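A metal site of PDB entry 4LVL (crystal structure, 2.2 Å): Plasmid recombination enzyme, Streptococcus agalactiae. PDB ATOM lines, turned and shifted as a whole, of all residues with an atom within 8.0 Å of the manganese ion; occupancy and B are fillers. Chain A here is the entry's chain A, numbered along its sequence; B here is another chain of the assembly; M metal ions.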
ATOM      1  N   HIS A  21     -22.729 -15.366   3.423  1.00  0.00           N
ATOM      2  CA  HIS A  21     -21.462 -16.004   3.729  1.00  0.00           C
ATOM      3  C   HIS A  21     -20.353 -14.940   3.850  1.00  0.00           C
ATOM      4  O   HIS A  21     -19.667 -14.893   4.865  1.00  0.00           O
ATOM      5  CB  HIS A  21     -21.112 -17.118   2.709  1.00  0.00           C
ATOM      6  CG  HIS A  21     -20.284 -18.231   3.291  1.00  0.00           C
ATOM      7  ND1 HIS A  21     -20.641 -18.909   4.447  1.00  0.00           N
ATOM      8  CD2 HIS A  21     -19.123 -18.792   2.879  1.00  0.00           C
ATOM      9  CE1 HIS A  21     -19.736 -19.837   4.711  1.00  0.00           C
ATOM     10  NE2 HIS A  21     -18.803 -19.773   3.782  1.00  0.00           N
ATOM     11  N   ASN A  22     -20.233 -14.083   2.836  1.00  0.00           N
ATOM     12  CA  ASN A  22     -19.158 -13.075   2.803  1.00  0.00           C
ATOM     13  C   ASN A  22     -19.156 -12.168   4.022  1.00  0.00           C
ATOM     14  O   ASN A  22     -18.091 -11.826   4.522  1.00  0.00           O
ATOM     15  CB  ASN A  22     -19.195 -12.152   1.567  1.00  0.00           C
ATOM     16  CG  ASN A  22     -18.796 -12.835   0.260  1.00  0.00           C
ATOM     17  OD1 ASN A  22     -18.500 -14.044   0.183  1.00  0.00           O
ATOM     18  ND2 ASN A  22     -18.849 -12.029  -0.818  1.00  0.00           N
ATOM     19  N   ARG A  24     -20.301 -13.061   6.889  1.00  0.00           N
ATOM     20  CA  ARG A  24     -20.312 -13.950   8.062  1.00  0.00           C
ATOM     21  C   ARG A  24     -21.488 -13.732   9.002  1.00  0.00           C
ATOM     22  O   ARG A  24     -21.290 -13.478  10.186  1.00  0.00           O
ATOM     23  CB  ARG A  24     -19.000 -13.857   8.842  1.00  0.00           C
ATOM     24  CG  ARG A  24     -17.795 -14.029   7.958  1.00  0.00           C
ATOM     25  CD  ARG A  24     -17.720 -15.487   7.570  1.00  0.00           C
ATOM     26  NE  ARG A  24     -16.405 -15.860   7.036  1.00  0.00           N
ATOM     27  CZ  ARG A  24     -16.217 -16.359   5.829  1.00  0.00           C
ATOM     28  NH1 ARG A  24     -17.240 -16.537   5.002  1.00  0.00           N
ATOM     29  NH2 ARG A  24     -15.007 -16.690   5.449  1.00  0.00           N
ATOM     30  N   ASN A  31     -18.429 -24.894   6.860  1.00  0.00           N
ATOM     31  CA  ASN A  31     -17.005 -24.933   6.558  1.00  0.00           C
ATOM     32  C   ASN A  31     -16.267 -25.047   7.896  1.00  0.00           C
ATOM     33  O   ASN A  31     -16.300 -24.120   8.698  1.00  0.00           O
ATOM     34  CB  ASN A  31     -16.579 -23.695   5.767  1.00  0.00           C
ATOM     35  CG  ASN A  31     -15.162 -23.781   5.217  1.00  0.00           C
ATOM     36  OD1 ASN A  31     -14.415 -24.711   5.544  1.00  0.00           O
ATOM     37  ND2 ASN A  31     -14.774 -22.822   4.385  1.00  0.00           N
ATOM     38  N   ILE A  34     -13.516 -22.352   8.609  1.00  0.00           N
ATOM     39  CA  ILE A  34     -13.697 -20.953   9.044  1.00  0.00           C
ATOM     40  C   ILE A  34     -13.419 -20.889  10.559  1.00  0.00           C
ATOM     41  O   ILE A  34     -13.971 -21.685  11.307  1.00  0.00           O
ATOM     42  CB  ILE A  34     -15.105 -20.360   8.726  1.00  0.00           C
ATOM     43  CG1 ILE A  34     -15.288 -20.141   7.230  1.00  0.00           C
ATOM     44  CG2 ILE A  34     -15.298 -19.007   9.423  1.00  0.00           C
ATOM     45  CD1 ILE A  34     -16.735 -20.160   6.780  1.00  0.00           C
ATOM     46  N   ASN A  42     -11.605  -9.934   9.304  1.00  0.00           N
ATOM     47  CA  ASN A  42     -11.995  -9.613   7.931  1.00  0.00           C
ATOM     48  C   ASN A  42     -12.265  -8.115   7.720  1.00  0.00           C
ATOM     49  O   ASN A  42     -12.509  -7.381   8.666  1.00  0.00           O
ATOM     50  CB  ASN A  42     -13.245 -10.404   7.533  1.00  0.00           C
ATOM     51  CG  ASN A  42     -13.036 -11.893   7.618  1.00  0.00           C
ATOM     52  OD1 ASN A  42     -11.898 -12.356   7.741  1.00  0.00           O
ATOM     53  ND2 ASN A  42     -14.142 -12.672   7.563  1.00  0.00           N
ATOM     54  N   GLU A  81     -17.959 -12.618  -9.633  1.00  0.00           N
ATOM     55  CA  GLU A  81     -17.226 -12.634  -8.372  1.00  0.00           C
ATOM     56  C   GLU A  81     -15.821 -13.226  -8.582  1.00  0.00           C
ATOM     57  O   GLU A  81     -15.652 -14.426  -8.900  1.00  0.00           O
ATOM     58  CB  GLU A  81     -17.983 -13.316  -7.220  1.00  0.00           C
ATOM     59  CG  GLU A  81     -17.215 -13.166  -5.894  1.00  0.00           C
ATOM     60  CD  GLU A  81     -17.835 -13.877  -4.701  1.00  0.00           C
ATOM     61  OE1 GLU A  81     -17.435 -15.028  -4.394  1.00  0.00           O
ATOM     62  OE2 GLU A  81     -18.710 -13.259  -4.042  1.00  0.00           O
ATOM     63  N   ILE A  83     -12.331 -14.347  -7.119  1.00  0.00           N
ATOM     64  CA  ILE A  83     -11.475 -14.746  -6.003  1.00  0.00           C
ATOM     65  C   ILE A  83     -10.054 -14.271  -6.326  1.00  0.00           C
ATOM     66  O   ILE A  83      -9.499 -14.607  -7.417  1.00  0.00           O
ATOM     67  CB  ILE A  83     -11.449 -16.281  -5.817  1.00  0.00           C
ATOM     68  CG1 ILE A  83     -12.846 -16.769  -5.462  1.00  0.00           C
ATOM     69  CG2 ILE A  83     -10.544 -16.663  -4.654  1.00  0.00           C
ATOM     70  CD1 ILE A  83     -13.346 -16.284  -4.121  1.00  0.00           C
ATOM     71  N   SER A 123     -14.546  -8.090  -0.330  1.00  0.00           N
ATOM     72  CA  SER A 123     -14.633  -8.626   1.020  1.00  0.00           C
ATOM     73  C   SER A 123     -13.357  -9.460   1.285  1.00  0.00           C
ATOM     74  O   SER A 123     -13.147 -10.518   0.660  1.00  0.00           O
ATOM     75  CB  SER A 123     -15.886  -9.530   1.057  1.00  0.00           C
ATOM     76  OG  SER A 123     -16.148 -10.027   2.351  1.00  0.00           O
ATOM     77  N   VAL A 124     -12.494  -9.004   2.198  1.00  0.00           N
ATOM     78  CA  VAL A 124     -11.219  -9.715   2.430  1.00  0.00           C
ATOM     79  C   VAL A 124     -11.347 -10.716   3.586  1.00  0.00           C
ATOM     80  O   VAL A 124     -11.614 -10.305   4.741  1.00  0.00           O
ATOM     81  CB  VAL A 124     -10.063  -8.725   2.709  1.00  0.00           C
ATOM     82  CG1 VAL A 124      -8.781  -9.513   3.029  1.00  0.00           C
ATOM     83  CG2 VAL A 124      -9.852  -7.805   1.503  1.00  0.00           C
ATOM     84  N   HIS A 125     -11.144 -12.009   3.312  1.00  0.00           N
ATOM     85  CA  HIS A 125     -11.264 -13.022   4.377  1.00  0.00           C
ATOM     86  C   HIS A 125      -9.923 -13.487   4.906  1.00  0.00           C
ATOM     87  O   HIS A 125      -9.114 -14.060   4.169  1.00  0.00           O
ATOM     88  CB  HIS A 125     -12.109 -14.217   3.946  1.00  0.00           C
ATOM     89  CG  HIS A 125     -13.536 -13.887   3.636  1.00  0.00           C
ATOM     90  ND1 HIS A 125     -14.403 -14.808   3.064  1.00  0.00           N
ATOM     91  CD2 HIS A 125     -14.258 -12.755   3.823  1.00  0.00           C
ATOM     92  CE1 HIS A 125     -15.597 -14.245   2.928  1.00  0.00           C
ATOM     93  NE2 HIS A 125     -15.532 -13.010   3.382  1.00  0.00           N
ATOM     94  N   LEU A 126      -9.729 -13.275   6.206  1.00  0.00           N
ATOM     95  CA  LEU A 126      -8.566 -13.706   6.948  1.00  0.00           C
ATOM     96  C   LEU A 126      -8.912 -14.823   7.966  1.00  0.00           C
ATOM     97  O   LEU A 126      -8.069 -15.233   8.773  1.00  0.00           O
ATOM     98  CB  LEU A 126      -7.926 -12.527   7.676  1.00  0.00           C
ATOM     99  CG  LEU A 126      -7.502 -11.333   6.817  1.00  0.00           C
ATOM    100  CD1 LEU A 126      -6.825 -10.342   7.741  1.00  0.00           C
ATOM    101  CD2 LEU A 126      -6.588 -11.733   5.696  1.00  0.00           C
ATOM    102  N   ASP A 127     -10.136 -15.297   7.940  1.00  0.00           N
ATOM    103  CA  ASP A 127     -10.582 -16.247   8.957  1.00  0.00           C
ATOM    104  C   ASP A 127     -10.665 -17.675   8.419  1.00  0.00           C
ATOM    105  O   ASP A 127     -11.299 -18.544   9.054  1.00  0.00           O
ATOM    106  CB  ASP A 127     -11.929 -15.799   9.532  1.00  0.00           C
ATOM    107  CG  ASP A 127     -13.082 -15.718   8.476  1.00  0.00           C
ATOM    108  OD1 ASP A 127     -12.880 -15.852   7.239  1.00  0.00           O
ATOM    109  OD2 ASP A 127     -14.247 -15.534   8.945  1.00  0.00           O
ATOM    110  N   GLU A 128     -10.067 -17.904   7.265  1.00  0.00           N
ATOM    111  CA  GLU A 128     -10.044 -19.226   6.607  1.00  0.00           C
ATOM    112  C   GLU A 128      -8.568 -19.650   6.447  1.00  0.00           C
ATOM    113  O   GLU A 128      -7.735 -19.148   7.182  1.00  0.00           O
ATOM    114  CB  GLU A 128     -10.792 -19.176   5.290  1.00  0.00           C
ATOM    115  CG  GLU A 128     -12.249 -18.880   5.528  1.00  0.00           C
ATOM    116  CD  GLU A 128     -13.041 -18.908   4.276  1.00  0.00           C
ATOM    117  OE1 GLU A 128     -13.602 -19.988   4.011  1.00  0.00           O
ATOM    118  OE2 GLU A 128     -13.090 -17.847   3.584  1.00  0.00           O
ATOM    119  N   SER A 129      -8.245 -20.542   5.510  1.00  0.00           N
ATOM    120  CA  SER A 129      -6.917 -21.143   5.460  1.00  0.00           C
ATOM    121  C   SER A 129      -5.837 -20.156   5.024  1.00  0.00           C
ATOM    122  O   SER A 129      -4.710 -20.187   5.555  1.00  0.00           O
ATOM    123  CB  SER A 129      -6.890 -22.326   4.509  1.00  0.00           C
ATOM    124  OG  SER A 129      -7.678 -23.406   4.983  1.00  0.00           O
ATOM    125  N   THR A 130      -6.206 -19.302   4.055  1.00  0.00           N
ATOM    126  CA  THR A 130      -5.286 -18.413   3.329  1.00  0.00           C
ATOM    127  C   THR A 130      -6.029 -17.100   3.086  1.00  0.00           C
ATOM    128  O   THR A 130      -7.212 -17.121   2.757  1.00  0.00           O
ATOM    129  CB  THR A 130      -4.886 -19.039   1.952  1.00  0.00           C
ATOM    130  OG1 THR A 130      -4.290 -20.325   2.158  1.00  0.00           O
ATOM    131  CG2 THR A 130      -3.896 -18.197   1.205  1.00  0.00           C
ATOM    132  N   PRO A 131      -5.331 -15.956   3.269  1.00  0.00           N
ATOM    133  CA  PRO A 131      -5.940 -14.680   2.948  1.00  0.00           C
ATOM    134  C   PRO A 131      -6.426 -14.677   1.490  1.00  0.00           C
ATOM    135  O   PRO A 131      -5.675 -15.085   0.585  1.00  0.00           O
ATOM    136  CB  PRO A 131      -4.793 -13.671   3.125  1.00  0.00           C
ATOM    137  CG  PRO A 131      -3.862 -14.306   4.115  1.00  0.00           C
ATOM    138  CD  PRO A 131      -4.038 -15.798   3.987  1.00  0.00           C
ATOM    139  N   HIS A 132      -7.671 -14.237   1.257  1.00  0.00           N
ATOM    140  CA  HIS A 132      -8.193 -14.104  -0.101  1.00  0.00           C
ATOM    141  C   HIS A 132      -9.280 -13.061  -0.067  1.00  0.00           C
ATOM    142  O   HIS A 132      -9.836 -12.794   1.009  1.00  0.00           O
ATOM    143  CB  HIS A 132      -8.768 -15.440  -0.640  1.00  0.00           C
ATOM    144  CG  HIS A 132      -9.862 -15.996   0.225  1.00  0.00           C
ATOM    145  ND1 HIS A 132      -9.594 -16.655   1.414  1.00  0.00           N
ATOM    146  CD2 HIS A 132     -11.213 -15.963   0.108  1.00  0.00           C
ATOM    147  CE1 HIS A 132     -10.731 -16.993   1.991  1.00  0.00           C
ATOM    148  NE2 HIS A 132     -11.725 -16.592   1.211  1.00  0.00           N
ATOM    149  N   MET A 133      -9.649 -12.539  -1.237  1.00  0.00           N
ATOM    150  CA  MET A 133     -10.702 -11.539  -1.371  1.00  0.00           C
ATOM    151  C   MET A 133     -11.807 -12.063  -2.281  1.00  0.00           C
ATOM    152  O   MET A 133     -11.479 -12.697  -3.295  1.00  0.00           O
ATOM    153  CB  MET A 133     -10.110 -10.242  -1.975  1.00  0.00           C
ATOM    154  CG  MET A 133     -11.145  -9.158  -2.240  1.00  0.00           C
ATOM    155  SD  MET A 133     -10.362  -7.576  -2.605  1.00  0.00           S
ATOM    156  CE  MET A 133      -9.447  -8.012  -4.086  1.00  0.00           C
ATOM    157  N   HIS A 134     -13.079 -11.811  -1.936  1.00  0.00           N
ATOM    158  CA  HIS A 134     -14.208 -12.023  -2.874  1.00  0.00           C
ATOM    159  C   HIS A 134     -14.585 -10.647  -3.409  1.00  0.00           C
ATOM    160  O   HIS A 134     -15.103  -9.795  -2.647  1.00  0.00           O
ATOM    161  CB  HIS A 134     -15.422 -12.577  -2.177  1.00  0.00           C
ATOM    162  CG  HIS A 134     -15.190 -13.866  -1.447  1.00  0.00           C
ATOM    163  ND1 HIS A 134     -15.678 -15.066  -1.902  1.00  0.00           N
ATOM    164  CD2 HIS A 134     -14.519 -14.133  -0.311  1.00  0.00           C
ATOM    165  CE1 HIS A 134     -15.302 -16.027  -1.073  1.00  0.00           C
ATOM    166  NE2 HIS A 134     -14.619 -15.486  -0.081  1.00  0.00           N
ATOM    167  N   VAL A 188     -14.331 -25.702  -3.890  1.00  0.00           N
ATOM    168  CA  VAL A 188     -13.680 -25.773  -2.601  1.00  0.00           C
ATOM    169  C   VAL A 188     -13.885 -27.147  -1.985  1.00  0.00           C
ATOM    170  O   VAL A 188     -12.930 -27.762  -1.510  1.00  0.00           O
ATOM    171  CB  VAL A 188     -14.160 -24.658  -1.637  1.00  0.00           C
ATOM    172  CG1 VAL A 188     -13.540 -24.820  -0.256  1.00  0.00           C
ATOM    173  CG2 VAL A 188     -13.787 -23.291  -2.213  1.00  0.00           C
ATOM    174  P    DG B  15     -10.871 -22.828   2.806  1.00  0.00           P
ATOM    175  OP1  DG B  15      -9.869 -22.363   3.773  1.00  0.00           O
ATOM    176  OP2  DG B  15     -12.166 -23.402   3.264  1.00  0.00           O
ATOM    177  O5'  DG B  15     -11.116 -21.550   1.875  1.00  0.00           O
ATOM    178  C5'  DG B  15     -12.265 -21.439   1.026  1.00  0.00           C
ATOM    179  C4'  DG B  15     -12.233 -20.120   0.290  1.00  0.00           C
ATOM    180  O4'  DG B  15     -11.517 -20.316  -0.940  1.00  0.00           O
ATOM    181  C3'  DG B  15     -13.604 -19.578  -0.111  1.00  0.00           C
ATOM    182  O3'  DG B  15     -14.094 -18.656   0.873  1.00  0.00           O
ATOM    183  C2'  DG B  15     -13.339 -18.896  -1.445  1.00  0.00           C
ATOM    184  C1'  DG B  15     -11.937 -19.336  -1.879  1.00  0.00           C
ATOM    185  N9   DG B  15     -11.879 -19.928  -3.215  1.00  0.00           N
ATOM    186  C8   DG B  15     -12.943 -20.280  -4.018  1.00  0.00           C
ATOM    187  N7   DG B  15     -12.582 -20.821  -5.146  1.00  0.00           N
ATOM    188  C5   DG B  15     -11.189 -20.857  -5.089  1.00  0.00           C
ATOM    189  C6   DG B  15     -10.231 -21.324  -6.028  1.00  0.00           C
ATOM    190  O6   DG B  15     -10.433 -21.847  -7.135  1.00  0.00           O
ATOM    191  N1   DG B  15      -8.933 -21.150  -5.571  1.00  0.00           N
ATOM    192  C2   DG B  15      -8.593 -20.612  -4.355  1.00  0.00           C
ATOM    193  N2   DG B  15      -7.271 -20.561  -4.079  1.00  0.00           N
ATOM    194  N3   DG B  15      -9.470 -20.178  -3.462  1.00  0.00           N
ATOM    195  C4   DG B  15     -10.739 -20.313  -3.895  1.00  0.00           C
ATOM    196  P   TS6 B  16     -15.550 -18.871   1.512  1.00  0.00           P
ATOM    197  S2P TS6 B  16     -16.661 -19.358   0.101  1.00  0.00           S
ATOM    198  O3P TS6 B  16     -15.946 -17.583   2.175  1.00  0.00           O
ATOM    199  O4P TS6 B  16     -15.683 -19.997   2.497  1.00  0.00           O
HETATM  200 MN    MN M   1     -13.852 -16.638   1.818  1.00  0.00          MN
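O3P of TS6 16 of chain B lies close to the guanidinium group (NH1) of Arg 24 (3.3 Å). ND2 of Asn 31 sits at hydrogen-bond distance from OP2 of DG 15 of chain B (2.9 Å). OP1 of DG 15 of chain B lies within hydrogen-bond range of the side-chain hydroxyl (OG) of Ser 129. The backbone carbonyl oxygen of His 21 is in hydrogen-bond range of the guanidinium group of Arg 24 (2.9 Å). A ring nitrogen (NE2) of His 125 sits at hydrogen-bond distance from the side-chain hydroxyl (OG) of Ser 123, at 3.2 Å. The guanidinium group of Arg 24 is in salt-bridge range of the side-chain carboxylate of Glu 128. O4P of TS6 16 of chain B is in hydrogen-bond range of a ring nitrogen (NE2) of His 21 (3.4 Å). O of Asn 22 is in hydrogen-bond range of NE2 of His 125 (3.0 Å).
The manganese ion is bound by NE2 of His 132, O3' of DG 15 of chain B, OE2 of Glu 128, ND1 of His 125, O3P of TS6 16 of chain B and NE2 of His 134.
Arg 24 touches the manganese ion. Within 4 Å of the manganese ion: Arg 24, His 125, Glu 128, His 132, His 134, DG 15 of chain B and TS6 16 of chain B.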
